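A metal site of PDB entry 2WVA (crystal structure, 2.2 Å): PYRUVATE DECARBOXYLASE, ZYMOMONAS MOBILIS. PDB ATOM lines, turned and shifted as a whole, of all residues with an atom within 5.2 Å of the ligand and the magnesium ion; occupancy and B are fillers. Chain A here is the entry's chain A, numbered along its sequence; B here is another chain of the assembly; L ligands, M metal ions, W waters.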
ATOM      1  N   GLU A 387       5.717   9.707  19.083  1.00  0.00           N
ATOM      2  CA  GLU A 387       4.371  10.176  19.391  1.00  0.00           C
ATOM      3  C   GLU A 387       3.950  11.423  18.616  1.00  0.00           C
ATOM      4  O   GLU A 387       4.779  12.253  18.267  1.00  0.00           O
ATOM      5  CB  GLU A 387       4.257  10.450  20.898  1.00  0.00           C
ATOM      6  CG  GLU A 387       2.872  10.851  21.382  1.00  0.00           C
ATOM      7  CD  GLU A 387       1.801   9.805  21.077  1.00  0.00           C
ATOM      8  OE1 GLU A 387       1.251   9.836  19.965  1.00  0.00           O
ATOM      9  OE2 GLU A 387       1.498   8.982  21.965  1.00  0.00           O
ATOM     10  N   THR A 388       2.655  11.551  18.355  1.00  0.00           N
ATOM     11  CA  THR A 388       2.113  12.799  17.842  1.00  0.00           C
ATOM     12  C   THR A 388       2.491  13.975  18.748  1.00  0.00           C
ATOM     13  O   THR A 388       2.340  13.926  19.976  1.00  0.00           O
ATOM     14  CB  THR A 388       0.586  12.730  17.782  1.00  0.00           C
ATOM     15  OG1 THR A 388       0.195  11.670  16.903  1.00  0.00           O
ATOM     16  CG2 THR A 388       0.000  14.076  17.309  1.00  0.00           C
ATOM     17  N   GLY A 389       2.967  15.049  18.121  1.00  0.00           N
ATOM     18  CA  GLY A 389       3.531  16.160  18.867  1.00  0.00           C
ATOM     19  C   GLY A 389       4.867  16.511  18.246  1.00  0.00           C
ATOM     20  O   GLY A 389       5.179  16.059  17.137  1.00  0.00           O
ATOM     21  N   ASP A 390       5.685  17.304  18.940  1.00  0.00           N
ATOM     22  CA  ASP A 390       6.944  17.713  18.349  1.00  0.00           C
ATOM     23  C   ASP A 390       7.838  16.496  18.101  1.00  0.00           C
ATOM     24  O   ASP A 390       8.776  16.571  17.300  1.00  0.00           O
ATOM     25  CB  ASP A 390       7.659  18.771  19.186  1.00  0.00           C
ATOM     26  CG  ASP A 390       8.638  19.603  18.362  1.00  0.00           C
ATOM     27  OD1 ASP A 390       8.393  19.797  17.145  1.00  0.00           O
ATOM     28  OD2 ASP A 390       9.655  20.082  18.912  1.00  0.00           O
ATOM     29  N   SER A 391       7.568  15.399  18.783  1.00  0.00           N
ATOM     30  CA  SER A 391       8.357  14.191  18.588  1.00  0.00           C
ATOM     31  C   SER A 391       8.268  13.708  17.132  1.00  0.00           C
ATOM     32  O   SER A 391       9.187  13.066  16.634  1.00  0.00           O
ATOM     33  CB  SER A 391       7.900  13.081  19.551  1.00  0.00           C
ATOM     34  OG  SER A 391       8.339  13.330  20.870  1.00  0.00           O
ATOM     35  N   GLY A 413      -3.287   9.422  14.635  1.00  0.00           N
ATOM     36  CA  GLY A 413      -2.754  10.532  15.420  1.00  0.00           C
ATOM     37  C   GLY A 413      -3.479  10.689  16.735  1.00  0.00           C
ATOM     38  O   GLY A 413      -3.844  11.805  17.140  1.00  0.00           O
ATOM     39  N   HIS A 414      -3.677   9.569  17.425  1.00  0.00           N
ATOM     40  CA  HIS A 414      -4.287   9.539  18.742  1.00  0.00           C
ATOM     41  C   HIS A 414      -3.182   9.738  19.756  1.00  0.00           C
ATOM     42  O   HIS A 414      -2.394   8.826  20.001  1.00  0.00           O
ATOM     43  CB  HIS A 414      -4.935   8.168  18.961  1.00  0.00           C
ATOM     44  CG  HIS A 414      -5.736   8.068  20.219  1.00  0.00           C
ATOM     45  ND1 HIS A 414      -5.161   8.162  21.461  1.00  0.00           N
ATOM     46  CD2 HIS A 414      -7.060   7.865  20.423  1.00  0.00           C
ATOM     47  CE1 HIS A 414      -6.100   8.038  22.389  1.00  0.00           C
ATOM     48  NE2 HIS A 414      -7.265   7.865  21.789  1.00  0.00           N
ATOM     49  N   ILE A 415      -3.091  10.913  20.382  1.00  0.00           N
ATOM     50  CA  ILE A 415      -2.046  11.101  21.379  1.00  0.00           C
ATOM     51  C   ILE A 415      -2.198  10.065  22.485  1.00  0.00           C
ATOM     52  O   ILE A 415      -3.331   9.758  22.913  1.00  0.00           O
ATOM     53  CB  ILE A 415      -1.966  12.537  21.966  1.00  0.00           C
ATOM     54  CG1 ILE A 415      -3.249  12.913  22.711  1.00  0.00           C
ATOM     55  CG2 ILE A 415      -1.664  13.546  20.891  1.00  0.00           C
ATOM     56  CD1 ILE A 415      -3.105  14.223  23.483  1.00  0.00           C
ATOM     57  N   GLY A 439       5.665  12.980  24.304  1.00  0.00           N
ATOM     58  CA  GLY A 439       5.454  14.218  25.029  1.00  0.00           C
ATOM     59  C   GLY A 439       4.695  14.025  26.321  1.00  0.00           C
ATOM     60  O   GLY A 439       3.999  13.029  26.508  1.00  0.00           O
ATOM     61  N   ASP A 440       4.835  14.980  27.233  1.00  0.00           N
ATOM     62  CA  ASP A 440       4.172  14.902  28.535  1.00  0.00           C
ATOM     63  C   ASP A 440       2.647  14.827  28.402  1.00  0.00           C
ATOM     64  O   ASP A 440       1.990  14.036  29.086  1.00  0.00           O
ATOM     65  CB  ASP A 440       4.588  16.069  29.452  1.00  0.00           C
ATOM     66  CG  ASP A 440       4.348  17.444  28.832  1.00  0.00           C
ATOM     67  OD1 ASP A 440       4.216  17.550  27.598  1.00  0.00           O
ATOM     68  OD2 ASP A 440       4.282  18.447  29.581  1.00  0.00           O
ATOM     69  N   GLY A 441       2.077  15.653  27.529  1.00  0.00           N
ATOM     70  CA  GLY A 441       0.633  15.674  27.320  1.00  0.00           C
ATOM     71  C   GLY A 441       0.085  14.340  26.835  1.00  0.00           C
ATOM     72  O   GLY A 441      -0.973  13.898  27.289  1.00  0.00           O
ATOM     73  N   SER A 442       0.795  13.702  25.903  1.00  0.00           N
ATOM     74  CA  SER A 442       0.354  12.421  25.348  1.00  0.00           C
ATOM     75  C   SER A 442       0.495  11.312  26.372  1.00  0.00           C
ATOM     76  O   SER A 442      -0.391  10.475  26.520  1.00  0.00           O
ATOM     77  CB  SER A 442       1.159  12.068  24.105  1.00  0.00           C
ATOM     78  OG  SER A 442       0.873  12.954  23.036  1.00  0.00           O
ATOM     79  N   PHE A 443       1.614  11.318  27.075  1.00  0.00           N
ATOM     80  CA  PHE A 443       1.878  10.333  28.102  1.00  0.00           C
ATOM     81  C   PHE A 443       0.730  10.226  29.112  1.00  0.00           C
ATOM     82  O   PHE A 443       0.410   9.137  29.582  1.00  0.00           O
ATOM     83  CB  PHE A 443       3.182  10.672  28.813  1.00  0.00           C
ATOM     84  CG  PHE A 443       3.660   9.620  29.759  1.00  0.00           C
ATOM     85  CD1 PHE A 443       4.296   8.493  29.282  1.00  0.00           C
ATOM     86  CD2 PHE A 443       3.476   9.749  31.131  1.00  0.00           C
ATOM     87  CE1 PHE A 443       4.747   7.510  30.139  1.00  0.00           C
ATOM     88  CE2 PHE A 443       3.932   8.771  32.001  1.00  0.00           C
ATOM     89  CZ  PHE A 443       4.575   7.647  31.512  1.00  0.00           C
ATOM     90  N   LEU A 445      -2.428  10.344  28.733  1.00  0.00           N
ATOM     91  CA  LEU A 445      -3.606   9.575  28.311  1.00  0.00           C
ATOM     92  C   LEU A 445      -3.527   8.091  28.627  1.00  0.00           C
ATOM     93  O   LEU A 445      -4.540   7.479  28.960  1.00  0.00           O
ATOM     94  CB  LEU A 445      -3.911   9.753  26.832  1.00  0.00           C
ATOM     95  CG  LEU A 445      -4.555  11.090  26.472  1.00  0.00           C
ATOM     96  CD1 LEU A 445      -3.465  12.105  26.178  1.00  0.00           C
ATOM     97  CD2 LEU A 445      -5.475  10.924  25.277  1.00  0.00           C
ATOM     98  N   ILE A 465       9.268  13.949  27.045  1.00  0.00           N
ATOM     99  CA  ILE A 465       9.597  15.354  26.820  1.00  0.00           C
ATOM    100  C   ILE A 465       8.660  16.236  27.646  1.00  0.00           C
ATOM    101  O   ILE A 465       7.492  16.425  27.279  1.00  0.00           O
ATOM    102  CB  ILE A 465       9.441  15.720  25.347  1.00  0.00           C
ATOM    103  CG1 ILE A 465      10.107  14.670  24.446  1.00  0.00           C
ATOM    104  CG2 ILE A 465      10.012  17.095  25.104  1.00  0.00           C
ATOM    105  CD1 ILE A 465      11.571  14.416  24.727  1.00  0.00           C
ATOM    106  N   ASN A 467       7.709  19.582  28.417  1.00  0.00           N
ATOM    107  CA  ASN A 467       7.712  21.002  28.106  1.00  0.00           C
ATOM    108  C   ASN A 467       6.447  21.655  28.669  1.00  0.00           C
ATOM    109  O   ASN A 467       6.009  22.708  28.224  1.00  0.00           O
ATOM    110  CB  ASN A 467       7.806  21.205  26.597  1.00  0.00           C
ATOM    111  CG  ASN A 467       6.724  20.477  25.860  1.00  0.00           C
ATOM    112  OD1 ASN A 467       5.817  19.927  26.483  1.00  0.00           O
ATOM    113  ND2 ASN A 467       6.801  20.455  24.520  1.00  0.00           N
ATOM    114  N   TYR A 468       5.840  20.964  29.629  1.00  0.00           N
ATOM    115  CA  TYR A 468       4.714  21.491  30.383  1.00  0.00           C
ATOM    116  C   TYR A 468       3.536  21.927  29.504  1.00  0.00           C
ATOM    117  O   TYR A 468       3.116  23.083  29.556  1.00  0.00           O
ATOM    118  CB  TYR A 468       5.181  22.629  31.304  1.00  0.00           C
ATOM    119  CG  TYR A 468       4.175  23.060  32.336  1.00  0.00           C
ATOM    120  CD1 TYR A 468       3.346  22.143  32.959  1.00  0.00           C
ATOM    121  CD2 TYR A 468       4.067  24.406  32.699  1.00  0.00           C
ATOM    122  CE1 TYR A 468       2.418  22.541  33.919  1.00  0.00           C
ATOM    123  CE2 TYR A 468       3.130  24.818  33.658  1.00  0.00           C
ATOM    124  CZ  TYR A 468       2.319  23.883  34.262  1.00  0.00           C
ATOM    125  OH  TYR A 468       1.398  24.284  35.210  1.00  0.00           O
ATOM    126  N   GLY A 469       3.012  21.004  28.691  1.00  0.00           N
ATOM    127  CA  GLY A 469       1.822  21.288  27.917  1.00  0.00           C
ATOM    128  C   GLY A 469       1.795  20.731  26.502  1.00  0.00           C
ATOM    129  O   GLY A 469       2.694  20.002  26.072  1.00  0.00           O
ATOM    130  N   TYR A 470       0.736  21.086  25.773  1.00  0.00           N
ATOM    131  CA  TYR A 470       0.529  20.621  24.397  1.00  0.00           C
ATOM    132  C   TYR A 470       1.214  21.535  23.348  1.00  0.00           C
ATOM    133  O   TYR A 470       0.531  22.320  22.691  1.00  0.00           O
ATOM    134  CB  TYR A 470      -0.966  20.614  24.083  1.00  0.00           C
ATOM    135  CG  TYR A 470      -1.840  19.733  24.935  1.00  0.00           C
ATOM    136  CD1 TYR A 470      -1.349  18.571  25.522  1.00  0.00           C
ATOM    137  CD2 TYR A 470      -3.196  20.026  25.118  1.00  0.00           C
ATOM    138  CE1 TYR A 470      -2.163  17.739  26.286  1.00  0.00           C
ATOM    139  CE2 TYR A 470      -4.015  19.203  25.873  1.00  0.00           C
ATOM    140  CZ  TYR A 470      -3.497  18.064  26.454  1.00  0.00           C
ATOM    141  OH  TYR A 470      -4.302  17.231  27.223  1.00  0.00           O
ATOM    142  N   THR A 471       2.521  21.402  23.158  1.00  0.00           N
ATOM    143  CA  THR A 471       3.243  22.341  22.264  1.00  0.00           C
ATOM    144  C   THR A 471       2.796  22.304  20.800  1.00  0.00           C
ATOM    145  O   THR A 471       2.651  23.348  20.174  1.00  0.00           O
ATOM    146  CB  THR A 471       4.790  22.189  22.375  1.00  0.00           C
ATOM    147  OG1 THR A 471       5.239  22.690  23.633  1.00  0.00           O
ATOM    148  CG2 THR A 471       5.496  22.959  21.256  1.00  0.00           C
ATOM    149  N   ILE A 472       2.575  21.111  20.249  1.00  0.00           N
ATOM    150  CA  ILE A 472       2.080  21.019  18.871  1.00  0.00           C
ATOM    151  C   ILE A 472       0.777  21.796  18.684  1.00  0.00           C
ATOM    152  O   ILE A 472       0.564  22.430  17.646  1.00  0.00           O
ATOM    153  CB  ILE A 472       1.887  19.525  18.407  1.00  0.00           C
ATOM    154  CG1 ILE A 472       1.426  19.458  16.945  1.00  0.00           C
ATOM    155  CG2 ILE A 472       0.920  18.772  19.335  1.00  0.00           C
ATOM    156  CD1 ILE A 472       1.475  18.067  16.354  1.00  0.00           C
ATOM    157  N   GLU A 473      -0.085  21.710  19.710  1.00  0.00           N
ATOM    158  CA  GLU A 473      -1.388  22.386  19.729  1.00  0.00           C
ATOM    159  C   GLU A 473      -1.193  23.895  19.856  1.00  0.00           C
ATOM    160  O   GLU A 473      -1.873  24.674  19.191  1.00  0.00           O
ATOM    161  CB  GLU A 473      -2.215  21.869  20.914  1.00  0.00           C
ATOM    162  CG  GLU A 473      -3.671  21.570  20.580  1.00  0.00           C
ATOM    163  CD  GLU A 473      -3.820  20.412  19.602  1.00  0.00           C
ATOM    164  OE1 GLU A 473      -4.700  19.565  19.824  1.00  0.00           O
ATOM    165  OE2 GLU A 473      -3.055  20.359  18.609  1.00  0.00           O
ATOM    166  N   VAL B  24     -11.286  17.940  26.187  1.00  0.00           N
ATOM    167  CA  VAL B  24      -9.914  17.643  25.792  1.00  0.00           C
ATOM    168  C   VAL B  24      -9.697  18.298  24.440  1.00  0.00           C
ATOM    169  O   VAL B  24     -10.402  17.991  23.481  1.00  0.00           O
ATOM    170  CB  VAL B  24      -9.656  16.127  25.657  1.00  0.00           C
ATOM    171  CG1 VAL B  24      -8.207  15.869  25.319  1.00  0.00           C
ATOM    172  CG2 VAL B  24     -10.046  15.414  26.963  1.00  0.00           C
ATOM    173  N   ALA B  25      -8.705  19.194  24.361  1.00  0.00           N
ATOM    174  CA  ALA B  25      -8.464  19.960  23.136  1.00  0.00           C
ATOM    175  C   ALA B  25      -8.028  19.088  21.967  1.00  0.00           C
ATOM    176  O   ALA B  25      -7.363  18.066  22.147  1.00  0.00           O
ATOM    177  CB  ALA B  25      -7.417  21.018  23.382  1.00  0.00           C
ATOM    178  N   GLY B  26      -8.388  19.511  20.757  1.00  0.00           N
ATOM    179  CA  GLY B  26      -7.894  18.921  19.527  1.00  0.00           C
ATOM    180  C   GLY B  26      -8.116  19.931  18.421  1.00  0.00           C
ATOM    181  O   GLY B  26      -9.047  20.731  18.484  1.00  0.00           O
ATOM    182  N   ASP B  27      -7.289  19.911  17.378  1.00  0.00           N
ATOM    183  CA  ASP B  27      -7.415  20.971  16.382  1.00  0.00           C
ATOM    184  C   ASP B  27      -8.831  21.113  15.784  1.00  0.00           C
ATOM    185  O   ASP B  27      -9.210  22.205  15.363  1.00  0.00           O
ATOM    186  CB  ASP B  27      -6.319  20.917  15.310  1.00  0.00           C
ATOM    187  CG  ASP B  27      -6.325  19.625  14.492  1.00  0.00           C
ATOM    188  OD1 ASP B  27      -7.013  18.647  14.867  1.00  0.00           O
ATOM    189  OD2 ASP B  27      -5.613  19.604  13.453  1.00  0.00           O
ATOM    190  N   GLU B  50     -10.143  11.139  26.756  1.00  0.00           N
ATOM    191  CA  GLU B  50     -11.541  11.338  26.400  1.00  0.00           C
ATOM    192  C   GLU B  50     -12.485  10.379  27.108  1.00  0.00           C
ATOM    193  O   GLU B  50     -13.652  10.717  27.327  1.00  0.00           O
ATOM    194  CB  GLU B  50     -11.751  11.320  24.894  1.00  0.00           C
ATOM    195  CG  GLU B  50     -11.197  12.535  24.184  1.00  0.00           C
ATOM    196  CD  GLU B  50      -9.695  12.436  23.950  1.00  0.00           C
ATOM    197  OE1 GLU B  50      -9.102  11.414  24.360  1.00  0.00           O
ATOM    198  OE2 GLU B  50      -9.113  13.378  23.332  1.00  0.00           O
ATOM    199  N   THR B  72     -12.370  15.893  20.421  1.00  0.00           N
ATOM    200  CA  THR B  72     -11.984  16.083  19.022  1.00  0.00           C
ATOM    201  C   THR B  72     -12.452  14.919  18.120  1.00  0.00           C
ATOM    202  O   THR B  72     -12.791  13.835  18.606  1.00  0.00           O
ATOM    203  CB  THR B  72     -10.478  16.331  18.891  1.00  0.00           C
ATOM    204  OG1 THR B  72     -10.196  16.813  17.575  1.00  0.00           O
ATOM    205  CG2 THR B  72      -9.679  15.051  19.133  1.00  0.00           C
ATOM    206  N   VAL B  75     -10.572  10.379  17.101  1.00  0.00           N
ATOM    207  CA  VAL B  75      -9.652   9.865  18.122  1.00  0.00           C
ATOM    208  C   VAL B  75     -10.163  10.231  19.521  1.00  0.00           C
ATOM    209  O   VAL B  75      -9.920   9.520  20.484  1.00  0.00           O
ATOM    210  CB  VAL B  75      -8.189  10.342  17.897  1.00  0.00           C
ATOM    211  CG1 VAL B  75      -7.597   9.675  16.660  1.00  0.00           C
ATOM    212  CG2 VAL B  75      -8.139  11.852  17.777  1.00  0.00           C
ATOM    213  N   GLY B  76     -10.898  11.332  19.607  1.00  0.00           N
ATOM    214  CA  GLY B  76     -11.510  11.737  20.856  1.00  0.00           C
ATOM    215  C   GLY B  76     -12.863  11.095  21.078  1.00  0.00           C
ATOM    216  O   GLY B  76     -13.140  10.516  22.140  1.00  0.00           O
ATOM    217  N   HIS B 114      -6.805  11.954  11.664  1.00  0.00           N
ATOM    218  CA  HIS B 114      -7.766  11.434  12.647  1.00  0.00           C
ATOM    219  C   HIS B 114      -8.917  10.619  12.075  1.00  0.00           C
ATOM    220  O   HIS B 114      -9.734  10.103  12.817  1.00  0.00           O
ATOM    221  CB  HIS B 114      -8.361  12.558  13.511  1.00  0.00           C
ATOM    222  CG  HIS B 114      -7.362  13.275  14.366  1.00  0.00           C
ATOM    223  ND1 HIS B 114      -6.115  12.754  14.668  1.00  0.00           N
ATOM    224  CD2 HIS B 114      -7.434  14.460  15.005  1.00  0.00           C
ATOM    225  CE1 HIS B 114      -5.457  13.604  15.422  1.00  0.00           C
ATOM    226  NE2 HIS B 114      -6.235  14.660  15.654  1.00  0.00           N
HETATM  227  O1  LIG L   1       5.926  18.105  21.986  1.00  0.00           O
HETATM  228  P1  LIG L   1       4.364  18.280  22.466  1.00  0.00           P
HETATM  229  O2  LIG L   1       3.440  18.849  21.220  1.00  0.00           O
HETATM  230  O3  LIG L   1       4.318  19.310  23.492  1.00  0.00           O
HETATM  231  O4  LIG L   1       3.838  16.813  23.005  1.00  0.00           O
HETATM  232  P2  LIG L   1       2.451  16.577  23.861  1.00  0.00           P
HETATM  233  O5  LIG L   1       2.730  16.930  25.428  1.00  0.00           O
HETATM  234  O6  LIG L   1       2.111  15.144  23.813  1.00  0.00           O
HETATM  235  O7  LIG L   1       1.213  17.470  23.278  1.00  0.00           O
HETATM  236  C1  LIG L   1       0.110  16.860  22.694  1.00  0.00           C
HETATM  237  C2  LIG L   1      -1.083  17.753  22.380  1.00  0.00           C
HETATM  238  C3  LIG L   1      -2.005  17.282  21.262  1.00  0.00           C
HETATM  239  C4  LIG L   1      -3.337  17.156  21.341  1.00  0.00           C
HETATM  240  C5  LIG L   1      -4.160  17.511  22.574  1.00  0.00           C
HETATM  241  N1  LIG L   1      -1.608  16.877  19.973  1.00  0.00           N
HETATM  242  N2  LIG L   1      -2.703  16.523  19.312  1.00  0.00           N
HETATM  243  N3  LIG L   1      -3.813  16.686  20.141  1.00  0.00           N
HETATM  244  C6  LIG L   1      -5.205  16.431  19.777  1.00  0.00           C
HETATM  245  C7  LIG L   1      -5.662  15.067  20.309  1.00  0.00           C
HETATM  246  C8  LIG L   1      -6.497  14.964  21.345  1.00  0.00           C
HETATM  247  N4  LIG L   1      -6.864  13.749  21.795  1.00  0.00           N
HETATM  248  C9  LIG L   1      -6.377  12.591  21.184  1.00  0.00           C
HETATM  249  C10 LIG L   1      -6.795  11.218  21.727  1.00  0.00           C
HETATM  250  N5  LIG L   1      -5.510  12.682  20.105  1.00  0.00           N
HETATM  251  C11 LIG L   1      -5.141  13.865  19.666  1.00  0.00           C
HETATM  252  N6  LIG L   1      -4.257  14.021  18.521  1.00  0.00           N
HETATM  253 MG    MG M   1       4.355  18.503  25.563  1.00  0.00          MG
HETATM  254  O   HOH W   1      -4.304  17.192  16.862  1.00  0.00           O
HETATM  255  O   HOH W   2       6.267  17.255  24.939  1.00  0.00           O
HETATM  256  O   HOH W   3       6.157  15.080  21.300  1.00  0.00           O
HETATM  257  O   HOH W   4       3.973  13.803  22.043  1.00  0.00           O
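Water W2 lies within hydrogen-bond range of O of Ile 465 (2.8 Å), O1 of the ligand (3.1 Å) and ND2 of Asn 467 (3.3 Å).
Water W4 lies within hydrogen-bond range of O of Thr 388, O6 of the ligand, N of Gly 439 and OG of Ser 442.
Water W1 bridges a nitrogen (N2) of the ligand (3.0 Å) and a ring nitrogen (NE2) of His 114 of chain B (3.4 Å).
Water W3 lies within hydrogen-bond range of the side-chain hydroxyl of Ser 391 (2.8 Å), an oxygen (O1) of the ligand (3.1 Å) and the backbone NH of Asp 390 (3.3 Å).
N3 of the ligand lies close to OE1 of Glu 473 (3.0 Å).
Merely in contact with the ligand: Gly 389 (3.6 Å), His 414 (3.3 Å), Gly 439 (3.6 Å), Leu 445 (3.8 Å), Tyr 470 (3.3 Å), Ala 25 of chain B (3.3 Å), Gly 26 of chain B (3.7 Å), Thr 72 of chain B (3.9 Å), Val 75 of chain B (3.6 Å) and His 114 of chain B (3.3 Å).
Hydrophobic or aromatic side chains that line the ligand: His 414, Ile 415, Leu 445, Tyr 470, Ile 472, Val 75 of chain B and His 114 of chain B.
Within 4 Å of the ligand: Gly 389, Asp 390, Gly 413, His 414, Ile 415, Gly 439, Asp 440, Gly 441, Ser 442, Leu 445, Asn 467, Gly 469, Tyr 470, Thr 471, Ile 472, Glu 473, Ala 25 of chain B, Gly 26 of chain B, Glu 50 of chain B, Thr 72 of chain B, Val 75 of chain B and His 114 of chain B.
Of the 31 residues printed, 3 come within 4 Å of the magnesium ion.
The nearest printed residue that does not touch the magnesium ion is Ile 465 (4.1 Å).
The backbone NH of Asp 440 sits at hydrogen-bond distance from the backbone carbonyl oxygen of Ile 465 (3.0 Å).
N of Tyr 468 sits at hydrogen-bond distance from OD2 of Asp 440, at 3.0 Å.
NE2 of His 414 sits close to O of Val 75 of chain B, at 3.4 Å.
The backbone carbonyl oxygen of Gly 413 sits close to a ring nitrogen (ND1) of His 114 of chain B, at 3.5 Å.
The side-chain amide nitrogen (ND2) of Asn 467 sits at hydrogen-bond distance from the side-chain hydroxyl (OG1) of Thr 471, at 2.9 Å.
The magnesium ion is bound by an oxygen (O3) of the ligand (2.2 Å).
The magnesium ion is bound by OD1 of Asn 467 (2.2 Å).
OD1 of Asp 440 is bound to the magnesium ion, 2.3 Å away.
The magnesium ion is bound by O5 of the ligand, 2.3 Å away.
O of Gly 469 is bound to the magnesium ion (2.3 Å).
The magnesium ion is bound by water W2, 2.4 Å away.
O6 of the ligand sits at hydrogen-bond distance from OG of Ser 442.
O6 of the ligand sits at hydrogen-bond distance from N of Ser 442 (2.9 Å).
O of Gly 413 lies within hydrogen-bond range of N6 of the ligand (2.6 Å).
The backbone NH (N) of Asp 440 sits close to an oxygen (O5) of the ligand (3.4 Å).
OE2 of Glu 50 of chain B lies within hydrogen-bond range of N4 of the ligand, at 2.7 Å.
O5 of the ligand sits close to N of Gly 441, 2.5 Å away.
The backbone NH (N) of Ile 472 is in hydrogen-bond range of an oxygen (O2) of the ligand (2.6 Å).
The backbone NH (N) of Ile 415 sits at hydrogen-bond distance from a nitrogen (N5) of the ligand (3.0 Å).
An oxygen (O2) of the ligand lies within hydrogen-bond range of the backbone NH (N) of Thr 471 (3.3 Å).
N of Asp 390 is in hydrogen-bond range of O1 of the ligand (3.2 Å).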
